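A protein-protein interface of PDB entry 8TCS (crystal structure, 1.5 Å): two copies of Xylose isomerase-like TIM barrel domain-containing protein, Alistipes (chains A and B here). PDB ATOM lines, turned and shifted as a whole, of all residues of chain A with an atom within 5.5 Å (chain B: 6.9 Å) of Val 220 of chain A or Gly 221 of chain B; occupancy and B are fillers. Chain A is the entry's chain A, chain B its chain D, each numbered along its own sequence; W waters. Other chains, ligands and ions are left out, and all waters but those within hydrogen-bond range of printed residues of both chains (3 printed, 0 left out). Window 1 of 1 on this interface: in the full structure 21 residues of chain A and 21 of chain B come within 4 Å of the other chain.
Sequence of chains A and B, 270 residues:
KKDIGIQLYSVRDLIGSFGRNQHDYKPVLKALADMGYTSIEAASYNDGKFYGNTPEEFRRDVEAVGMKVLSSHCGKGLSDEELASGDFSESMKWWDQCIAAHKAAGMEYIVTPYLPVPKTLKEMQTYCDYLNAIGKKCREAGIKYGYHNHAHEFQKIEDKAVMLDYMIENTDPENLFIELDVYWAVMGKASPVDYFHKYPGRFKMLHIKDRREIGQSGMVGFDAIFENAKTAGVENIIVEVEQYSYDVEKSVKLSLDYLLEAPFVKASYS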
ATOM      1  N   VAL A 182      20.006  34.830 -13.409  1.00  0.00           N
ATOM      2  CA  VAL A 182      20.602  33.704 -12.714  1.00  0.00           C
ATOM      3  C   VAL A 182      20.457  32.404 -13.494  1.00  0.00           C
ATOM      4  O   VAL A 182      21.367  31.581 -13.463  1.00  0.00           O
ATOM      5  CB  VAL A 182      20.077  33.631 -11.277  1.00  0.00           C
ATOM      6  CG1 VAL A 182      20.513  34.877 -10.511  1.00  0.00           C
ATOM      7  CG2 VAL A 182      18.591  33.384 -11.208  1.00  0.00           C
ATOM      8  N   TYR A 183      19.392  32.226 -14.280  1.00  0.00           N
ATOM      9  CA  TYR A 183      19.267  31.043 -15.130  1.00  0.00           C
ATOM     10  C   TYR A 183      20.298  31.068 -16.232  1.00  0.00           C
ATOM     11  O   TYR A 183      20.995  30.066 -16.468  1.00  0.00           O
ATOM     12  CB  TYR A 183      17.851  30.958 -15.687  1.00  0.00           C
ATOM     13  CG  TYR A 183      17.710  29.853 -16.727  1.00  0.00           C
ATOM     14  CD1 TYR A 183      17.548  28.527 -16.331  1.00  0.00           C
ATOM     15  CD2 TYR A 183      17.664  30.130 -18.084  1.00  0.00           C
ATOM     16  CE1 TYR A 183      17.359  27.526 -17.266  1.00  0.00           C
ATOM     17  CE2 TYR A 183      17.495  29.131 -19.019  1.00  0.00           C
ATOM     18  CZ  TYR A 183      17.329  27.829 -18.614  1.00  0.00           C
ATOM     19  OH  TYR A 183      17.101  26.840 -19.524  1.00  0.00           O
ATOM     20  N   VAL A 186      23.727  30.220 -14.979  1.00  0.00           N
ATOM     21  CA  VAL A 186      23.935  28.777 -14.791  1.00  0.00           C
ATOM     22  C   VAL A 186      24.126  28.085 -16.123  1.00  0.00           C
ATOM     23  O   VAL A 186      25.011  27.230 -16.316  1.00  0.00           O
ATOM     24  CB  VAL A 186      22.781  28.215 -13.963  1.00  0.00           C
ATOM     25  CG1 VAL A 186      22.850  26.701 -13.926  1.00  0.00           C
ATOM     26  CG2 VAL A 186      22.808  28.812 -12.575  1.00  0.00           C
ATOM     27  N   LYS A 209      14.790  33.925 -12.985  1.00  0.00           N
ATOM     28  CA  LYS A 209      14.390  33.167 -14.143  1.00  0.00           C
ATOM     29  C   LYS A 209      14.786  31.717 -13.879  1.00  0.00           C
ATOM     30  O   LYS A 209      15.751  31.451 -13.185  1.00  0.00           O
ATOM     31  CB  LYS A 209      15.051  33.700 -15.409  1.00  0.00           C
ATOM     32  CG  LYS A 209      14.541  32.997 -16.670  1.00  0.00           C
ATOM     33  CD  LYS A 209      15.134  33.472 -17.975  1.00  0.00           C
ATOM     34  CE  LYS A 209      14.504  32.738 -19.137  1.00  0.00           C
ATOM     35  NZ  LYS A 209      14.527  31.281 -18.985  1.00  0.00           N
ATOM     36  N   ASP A 210      14.006  30.800 -14.468  1.00  0.00           N
ATOM     37  CA  ASP A 210      14.276  29.363 -14.467  1.00  0.00           C
ATOM     38  C   ASP A 210      13.993  28.849 -15.877  1.00  0.00           C
ATOM     39  O   ASP A 210      13.838  29.607 -16.826  1.00  0.00           O
ATOM     40  CB  ASP A 210      13.511  28.691 -13.351  1.00  0.00           C
ATOM     41  CG  ASP A 210      14.068  27.376 -12.799  1.00  0.00           C
ATOM     42  OD1 ASP A 210      14.853  26.755 -13.528  1.00  0.00           O
ATOM     43  OD2 ASP A 210      13.706  27.006 -11.649  1.00  0.00           O
ATOM     44  N   SER A 217      12.715  23.505 -11.889  1.00  0.00           N
ATOM     45  CA  SER A 217      13.546  22.686 -12.771  1.00  0.00           C
ATOM     46  C   SER A 217      14.620  21.881 -12.047  1.00  0.00           C
ATOM     47  O   SER A 217      15.135  20.900 -12.599  1.00  0.00           O
ATOM     48  CB  SER A 217      14.253  23.518 -13.823  1.00  0.00           C
ATOM     49  OG  SER A 217      15.276  24.309 -13.243  1.00  0.00           O
ATOM     50  N   GLY A 218      15.085  22.404 -10.921  1.00  0.00           N
ATOM     51  CA  GLY A 218      16.259  21.829 -10.275  1.00  0.00           C
ATOM     52  C   GLY A 218      17.572  22.459 -10.756  1.00  0.00           C
ATOM     53  O   GLY A 218      18.639  22.044 -10.307  1.00  0.00           O
ATOM     54  N   MET A 219      17.523  23.452 -11.674  1.00  0.00           N
ATOM     55  CA  MET A 219      18.736  23.991 -12.274  1.00  0.00           C
ATOM     56  C   MET A 219      19.240  25.274 -11.604  1.00  0.00           C
ATOM     57  O   MET A 219      20.324  25.727 -11.987  1.00  0.00           O
ATOM     58  CB  MET A 219      18.534  24.307 -13.758  1.00  0.00           C
ATOM     59  CG  MET A 219      18.088  23.121 -14.569  1.00  0.00           C
ATOM     60  SD  MET A 219      18.030  23.432 -16.343  1.00  0.00           S
ATOM     61  CE  MET A 219      19.798  23.559 -16.655  1.00  0.00           C
ATOM     62  N   VAL A 220      18.463  25.902 -10.732  1.00  0.00           N
ATOM     63  CA  VAL A 220      18.885  27.159 -10.124  1.00  0.00           C
ATOM     64  C   VAL A 220      18.737  27.100  -8.603  1.00  0.00           C
ATOM     65  O   VAL A 220      17.660  26.817  -8.055  1.00  0.00           O
ATOM     66  CB  VAL A 220      18.067  28.347 -10.692  1.00  0.00           C
ATOM     67  CG1 VAL A 220      18.593  29.690 -10.178  1.00  0.00           C
ATOM     68  CG2 VAL A 220      18.121  28.367 -12.195  1.00  0.00           C
ATOM     69  N   GLY A 221      19.842  27.460  -7.934  1.00  0.00           N
ATOM     70  CA  GLY A 221      19.900  27.424  -6.477  1.00  0.00           C
ATOM     71  C   GLY A 221      19.437  28.749  -5.856  1.00  0.00           C
ATOM     72  O   GLY A 221      20.250  29.541  -5.369  1.00  0.00           O
ATOM     73  N   PHE A 222      18.130  29.031  -5.895  1.00  0.00           N
ATOM     74  CA  PHE A 222      17.617  30.304  -5.398  1.00  0.00           C
ATOM     75  C   PHE A 222      17.971  30.518  -3.925  1.00  0.00           C
ATOM     76  O   PHE A 222      18.297  31.637  -3.533  1.00  0.00           O
ATOM     77  CB  PHE A 222      16.114  30.415  -5.665  1.00  0.00           C
ATOM     78  CG  PHE A 222      15.792  30.450  -7.157  1.00  0.00           C
ATOM     79  CD1 PHE A 222      16.050  31.587  -7.917  1.00  0.00           C
ATOM     80  CD2 PHE A 222      15.227  29.357  -7.797  1.00  0.00           C
ATOM     81  CE1 PHE A 222      15.802  31.587  -9.264  1.00  0.00           C
ATOM     82  CE2 PHE A 222      14.925  29.401  -9.148  1.00  0.00           C
ATOM     83  CZ  PHE A 222      15.232  30.508  -9.875  1.00  0.00           C
ATOM     84  N   ILE A 225      21.445  31.969  -3.837  1.00  0.00           N
ATOM     85  CA  ILE A 225      21.426  33.294  -4.443  1.00  0.00           C
ATOM     86  C   ILE A 225      20.899  34.331  -3.437  1.00  0.00           C
ATOM     87  O   ILE A 225      21.565  35.377  -3.221  1.00  0.00           O
ATOM     88  CB  ILE A 225      20.614  33.263  -5.756  1.00  0.00           C
ATOM     89  CG1 ILE A 225      21.361  32.428  -6.798  1.00  0.00           C
ATOM     90  CG2 ILE A 225      20.321  34.677  -6.227  1.00  0.00           C
ATOM     91  CD1 ILE A 225      20.493  31.932  -7.962  1.00  0.00           C
ATOM     92  N   TYR A 258       6.101  30.709  -5.534  1.00  0.00           N
ATOM     93  CA  TYR A 258       7.348  30.115  -5.091  1.00  0.00           C
ATOM     94  C   TYR A 258       8.136  31.117  -4.250  1.00  0.00           C
ATOM     95  O   TYR A 258       8.612  30.781  -3.171  1.00  0.00           O
ATOM     96  CB  TYR A 258       8.172  29.594  -6.264  1.00  0.00           C
ATOM     97  CG  TYR A 258       9.589  29.155  -5.866  1.00  0.00           C
ATOM     98  CD1 TYR A 258       9.866  27.869  -5.421  1.00  0.00           C
ATOM     99  CD2 TYR A 258      10.653  30.057  -5.896  1.00  0.00           C
ATOM    100  CE1 TYR A 258      11.146  27.481  -5.037  1.00  0.00           C
ATOM    101  CE2 TYR A 258      11.939  29.663  -5.569  1.00  0.00           C
ATOM    102  CZ  TYR A 258      12.194  28.367  -5.154  1.00  0.00           C
ATOM    103  OH  TYR A 258      13.467  28.019  -4.816  1.00  0.00           O
ATOM    104  N   VAL B 186      23.121  19.633 -14.643  1.00  0.00           N
ATOM    105  CA  VAL B 186      22.948  21.075 -14.845  1.00  0.00           C
ATOM    106  C   VAL B 186      24.035  21.612 -15.783  1.00  0.00           C
ATOM    107  O   VAL B 186      23.755  22.434 -16.683  1.00  0.00           O
ATOM    108  CB  VAL B 186      22.854  21.841 -13.521  1.00  0.00           C
ATOM    109  CG1 VAL B 186      22.986  23.334 -13.743  1.00  0.00           C
ATOM    110  CG2 VAL B 186      21.570  21.483 -12.753  1.00  0.00           C
ATOM    111  N   PRO B 192      17.272  18.231 -13.881  1.00  0.00           N
ATOM    112  CA  PRO B 192      17.046  17.000 -13.122  1.00  0.00           C
ATOM    113  C   PRO B 192      15.567  16.653 -13.006  1.00  0.00           C
ATOM    114  O   PRO B 192      15.203  15.502 -13.199  1.00  0.00           O
ATOM    115  CB  PRO B 192      17.698  17.300 -11.763  1.00  0.00           C
ATOM    116  CG  PRO B 192      18.815  18.235 -12.132  1.00  0.00           C
ATOM    117  CD  PRO B 192      18.152  19.181 -13.184  1.00  0.00           C
ATOM    118  N   VAL B 193      14.718  17.636 -12.686  1.00  0.00           N
ATOM    119  CA  VAL B 193      13.307  17.347 -12.485  1.00  0.00           C
ATOM    120  C   VAL B 193      12.662  16.919 -13.794  1.00  0.00           C
ATOM    121  O   VAL B 193      11.839  15.974 -13.799  1.00  0.00           O
ATOM    122  CB  VAL B 193      12.620  18.590 -11.899  1.00  0.00           C
ATOM    123  CG1 VAL B 193      11.102  18.414 -11.824  1.00  0.00           C
ATOM    124  CG2 VAL B 193      13.187  18.903 -10.527  1.00  0.00           C
ATOM    125  N   GLY B 218      24.626  28.471  -5.976  1.00  0.00           N
ATOM    126  CA  GLY B 218      23.510  29.009  -6.751  1.00  0.00           C
ATOM    127  C   GLY B 218      23.212  28.225  -8.037  1.00  0.00           C
ATOM    128  O   GLY B 218      22.288  28.585  -8.781  1.00  0.00           O
ATOM    129  N   MET B 219      23.958  27.168  -8.345  1.00  0.00           N
ATOM    130  CA  MET B 219      23.843  26.469  -9.607  1.00  0.00           C
ATOM    131  C   MET B 219      22.990  25.210  -9.531  1.00  0.00           C
ATOM    132  O   MET B 219      22.754  24.607 -10.576  1.00  0.00           O
ATOM    133  CB  MET B 219      25.204  26.043 -10.140  1.00  0.00           C
ATOM    134  CG  MET B 219      26.192  27.168 -10.344  1.00  0.00           C
ATOM    135  SD  MET B 219      27.726  26.649 -11.119  1.00  0.00           S
ATOM    136  CE  MET B 219      27.231  26.219 -12.806  1.00  0.00           C
ATOM    137  N   VAL B 220      22.540  24.804  -8.347  1.00  0.00           N
ATOM    138  CA  VAL B 220      21.725  23.601  -8.276  1.00  0.00           C
ATOM    139  C   VAL B 220      20.516  23.861  -7.385  1.00  0.00           C
ATOM    140  O   VAL B 220      20.612  24.262  -6.229  1.00  0.00           O
ATOM    141  CB  VAL B 220      22.521  22.371  -7.780  1.00  0.00           C
ATOM    142  CG1 VAL B 220      21.633  21.128  -7.753  1.00  0.00           C
ATOM    143  CG2 VAL B 220      23.766  22.127  -8.599  1.00  0.00           C
ATOM    144  N   GLY B 221      19.331  23.565  -7.929  1.00  0.00           N
ATOM    145  CA  GLY B 221      18.091  23.760  -7.225  1.00  0.00           C
ATOM    146  C   GLY B 221      17.699  22.503  -6.447  1.00  0.00           C
ATOM    147  O   GLY B 221      16.818  21.737  -6.848  1.00  0.00           O
ATOM    148  N   PHE B 222      18.387  22.305  -5.315  1.00  0.00           N
ATOM    149  CA  PHE B 222      18.155  21.151  -4.467  1.00  0.00           C
ATOM    150  C   PHE B 222      16.716  21.094  -3.974  1.00  0.00           C
ATOM    151  O   PHE B 222      16.151  19.999  -3.895  1.00  0.00           O
ATOM    152  CB  PHE B 222      19.152  21.127  -3.290  1.00  0.00           C
ATOM    153  CG  PHE B 222      20.573  20.875  -3.755  1.00  0.00           C
ATOM    154  CD1 PHE B 222      20.975  19.637  -4.256  1.00  0.00           C
ATOM    155  CD2 PHE B 222      21.512  21.908  -3.745  1.00  0.00           C
ATOM    156  CE1 PHE B 222      22.267  19.424  -4.695  1.00  0.00           C
ATOM    157  CE2 PHE B 222      22.811  21.678  -4.184  1.00  0.00           C
ATOM    158  CZ  PHE B 222      23.200  20.443  -4.642  1.00  0.00           C
ATOM    159  N   ASP B 223      16.086  22.243  -3.658  1.00  0.00           N
ATOM    160  CA  ASP B 223      14.701  22.211  -3.216  1.00  0.00           C
ATOM    161  C   ASP B 223      13.811  21.483  -4.231  1.00  0.00           C
ATOM    162  O   ASP B 223      13.035  20.590  -3.854  1.00  0.00           O
ATOM    163  CB  ASP B 223      14.191  23.597  -2.845  1.00  0.00           C
ATOM    164  CG  ASP B 223      14.276  24.686  -3.916  1.00  0.00           C
ATOM    165  OD1 ASP B 223      14.929  24.441  -4.972  1.00  0.00           O
ATOM    166  OD2 ASP B 223      13.754  25.815  -3.634  1.00  0.00           O
ATOM    167  N   ALA B 224      13.926  21.816  -5.519  1.00  0.00           N
ATOM    168  CA  ALA B 224      13.056  21.230  -6.541  1.00  0.00           C
ATOM    169  C   ALA B 224      13.392  19.752  -6.718  1.00  0.00           C
ATOM    170  O   ALA B 224      12.510  18.911  -7.010  1.00  0.00           O
ATOM    171  CB  ALA B 224      13.174  21.962  -7.843  1.00  0.00           C
ATOM    172  N   ILE B 225      14.687  19.432  -6.614  1.00  0.00           N
ATOM    173  CA  ILE B 225      15.136  18.054  -6.801  1.00  0.00           C
ATOM    174  C   ILE B 225      14.516  17.162  -5.717  1.00  0.00           C
ATOM    175  O   ILE B 225      13.892  16.127  -6.017  1.00  0.00           O
ATOM    176  CB  ILE B 225      16.682  18.011  -6.824  1.00  0.00           C
ATOM    177  CG1 ILE B 225      17.205  18.613  -8.115  1.00  0.00           C
ATOM    178  CG2 ILE B 225      17.216  16.602  -6.611  1.00  0.00           C
ATOM    179  CD1 ILE B 225      18.662  18.983  -8.063  1.00  0.00           C
ATOM    180  N   PHE B 226      14.612  17.575  -4.455  1.00  0.00           N
ATOM    181  CA  PHE B 226      14.088  16.778  -3.351  1.00  0.00           C
ATOM    182  C   PHE B 226      12.558  16.736  -3.374  1.00  0.00           C
ATOM    183  O   PHE B 226      11.996  15.703  -3.055  1.00  0.00           O
ATOM    184  CB  PHE B 226      14.636  17.281  -2.021  1.00  0.00           C
ATOM    185  CG  PHE B 226      16.052  16.786  -1.794  1.00  0.00           C
ATOM    186  CD1 PHE B 226      16.261  15.494  -1.344  1.00  0.00           C
ATOM    187  CD2 PHE B 226      17.158  17.548  -2.142  1.00  0.00           C
ATOM    188  CE1 PHE B 226      17.536  15.015  -1.142  1.00  0.00           C
ATOM    189  CE2 PHE B 226      18.442  17.055  -1.966  1.00  0.00           C
ATOM    190  CZ  PHE B 226      18.621  15.771  -1.464  1.00  0.00           C
ATOM    191  N   TYR B 258      24.260  21.508   5.297  1.00  0.00           N
ATOM    192  CA  TYR B 258      23.240  22.098   4.433  1.00  0.00           C
ATOM    193  C   TYR B 258      22.056  21.143   4.351  1.00  0.00           C
ATOM    194  O   TYR B 258      20.880  21.493   4.475  1.00  0.00           O
ATOM    195  CB  TYR B 258      23.838  22.362   3.060  1.00  0.00           C
ATOM    196  CG  TYR B 258      22.808  22.758   2.016  1.00  0.00           C
ATOM    197  CD1 TYR B 258      22.370  24.077   1.864  1.00  0.00           C
ATOM    198  CD2 TYR B 258      22.272  21.799   1.188  1.00  0.00           C
ATOM    199  CE1 TYR B 258      21.450  24.413   0.877  1.00  0.00           C
ATOM    200  CE2 TYR B 258      21.359  22.112   0.202  1.00  0.00           C
ATOM    201  CZ  TYR B 258      20.927  23.426   0.062  1.00  0.00           C
ATOM    202  OH  TYR B 258      20.014  23.704  -0.918  1.00  0.00           O
ATOM    203  N   PHE B 264      13.410  20.184   3.113  1.00  0.00           N
ATOM    204  CA  PHE B 264      12.960  19.365   1.995  1.00  0.00           C
ATOM    205  C   PHE B 264      13.721  18.031   1.864  1.00  0.00           C
ATOM    206  O   PHE B 264      13.331  17.173   1.062  1.00  0.00           O
ATOM    207  CB  PHE B 264      13.087  20.195   0.704  1.00  0.00           C
ATOM    208  CG  PHE B 264      14.420  20.869   0.473  1.00  0.00           C
ATOM    209  CD1 PHE B 264      15.516  20.131   0.042  1.00  0.00           C
ATOM    210  CD2 PHE B 264      14.573  22.249   0.651  1.00  0.00           C
ATOM    211  CE1 PHE B 264      16.726  20.740  -0.189  1.00  0.00           C
ATOM    212  CE2 PHE B 264      15.811  22.855   0.462  1.00  0.00           C
ATOM    213  CZ  PHE B 264      16.899  22.090   0.072  1.00  0.00           C
HETATM  214  O   HOH W   1      14.994  25.923  -7.330  1.00  0.00           O
HETATM  215  O   HOH W   2      24.984  24.708 -17.700  1.00  0.00           O
HETATM  216  O   HOH W   3      16.646  26.977  -3.992  1.00  0.00           O
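The backbone NH (N) of Val 193 of chain B sits at hydrogen-bond distance from the backbone carbonyl oxygen (O) of Ser 217 of chain A (3.3 Å). The backbone carbonyl oxygen (O) of Met 219 of chain A sits close to the backbone carbonyl oxygen (O) of Met 219 of chain B, at 3.0 Å. The side-chain hydroxyl (OH) of Tyr 258 of chain A lies within hydrogen-bond range of the side-chain carboxylate (OD2) of Asp 223 of chain B. The backbone carbonyl oxygen (O) of Gly 218 of chain A lies within hydrogen-bond range of the backbone NH (N) of Gly 221 of chain B, at 2.9 Å. O of Gly 218 of chain B is in hydrogen-bond range of N of Gly 221 of chain A (2.8 Å).
OG of Ser 217 of chain A sits at hydrogen-bond distance from OD1 of Asp 210 of chain A (2.5 Å). N of Met 219 of chain A sits at hydrogen-bond distance from OG of Ser 217 of chain A, 2.9 Å away.
CG2 of Val 186 of chain A touches CA of Met 219 of chain B, at 3.9 Å. Pro 192 of chain B touches Ser 217 of chain A. Gly 218 of chain A touches Val 186 of chain B (O to CG2, 3.9 Å). Gly 218 of chain A touches Val 220 of chain B. CD1 of Ile 225 of chain B touches O of Gly 218 of chain A, 3.8 Å away. CA of Met 219 of chain A touches CG2 of Val 186 of chain B, 3.8 Å away. Val 220 of chain A touches Gly 221 of chain B. CA of Gly 221 of chain A touches O of Val 220 of chain B, 3.3 Å away. Gly 221 of chain A touches Gly 221 of chain B (N to N, 3.9 Å). Gly 218 of chain B touches Ile 225 of chain A (O to CD1, 3.9 Å).
Of chain A, only Gly 218, Val 220 and Gly 221 come within 4 Å of Gly 221 of chain B. Of the printed residues of chain A, Asp 223 of chain B touches Tyr 258. Printed residues of chain B within 4 Å of Ile 225 of chain A: Gly 218. Printed residues of chain A within 4 Å of Ile 225 of chain B: Gly 218. Printed residues of chain B within 4 Å of Tyr 258 of chain A: Asp 223. Lys 209 of chain A touches none of the printed residues of chain B.
Printed residues of chain A that touch a printed residue of chain B: Val 186, Ser 217, Gly 218, Met 219, Val 220, Gly 221, Ile 225 and Tyr 258. Hydrophobic or aromatic side chains of chain A that line the printed part of chain B: Val 186, Ile 225 and Tyr 258.
Val 186 of chain B touches its own counterpart, Val 186 of chain A. Val 186 of chain A touches Gly 218 of chain B, and with the chains exchanged Gly 218 of chain A touches Val 186 of chain B. Val 186 of chain A touches Met 219 of chain B, and with the chains exchanged Met 219 of chain A touches Val 186 of chain B. Gly 218 of chain A touches Ile 225 of chain B, and with the chains exchanged Ile 225 of chain A touches Gly 218 of chain B. Positions printed for both chains: 186, 218, 219, 220, 221, 222, 225 and 258. Of the 20 pairs that touch across the chains among the printed residues, 16 have their exchanged pair printed and touching as well.
Water W2 lies within hydrogen-bond range of the backbone carbonyl oxygen (O) of Val 186 of chain B (2.8 Å) and the backbone carbonyl oxygen (O) of Val 186 of chain A (2.9 Å). Water W1 lies within hydrogen-bond range of the side-chain carboxylate of Asp 223 of chain B (2.8 Å) and the backbone carbonyl oxygen of Val 220 of chain A (2.9 Å). Water W3 lies within hydrogen-bond range of the side-chain carboxylate of Asp 223 of chain B (3.1 Å), the backbone NH of Phe 222 of chain A (3.2 Å) and the side-chain hydroxyl of Tyr 258 of chain A (3.4 Å).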
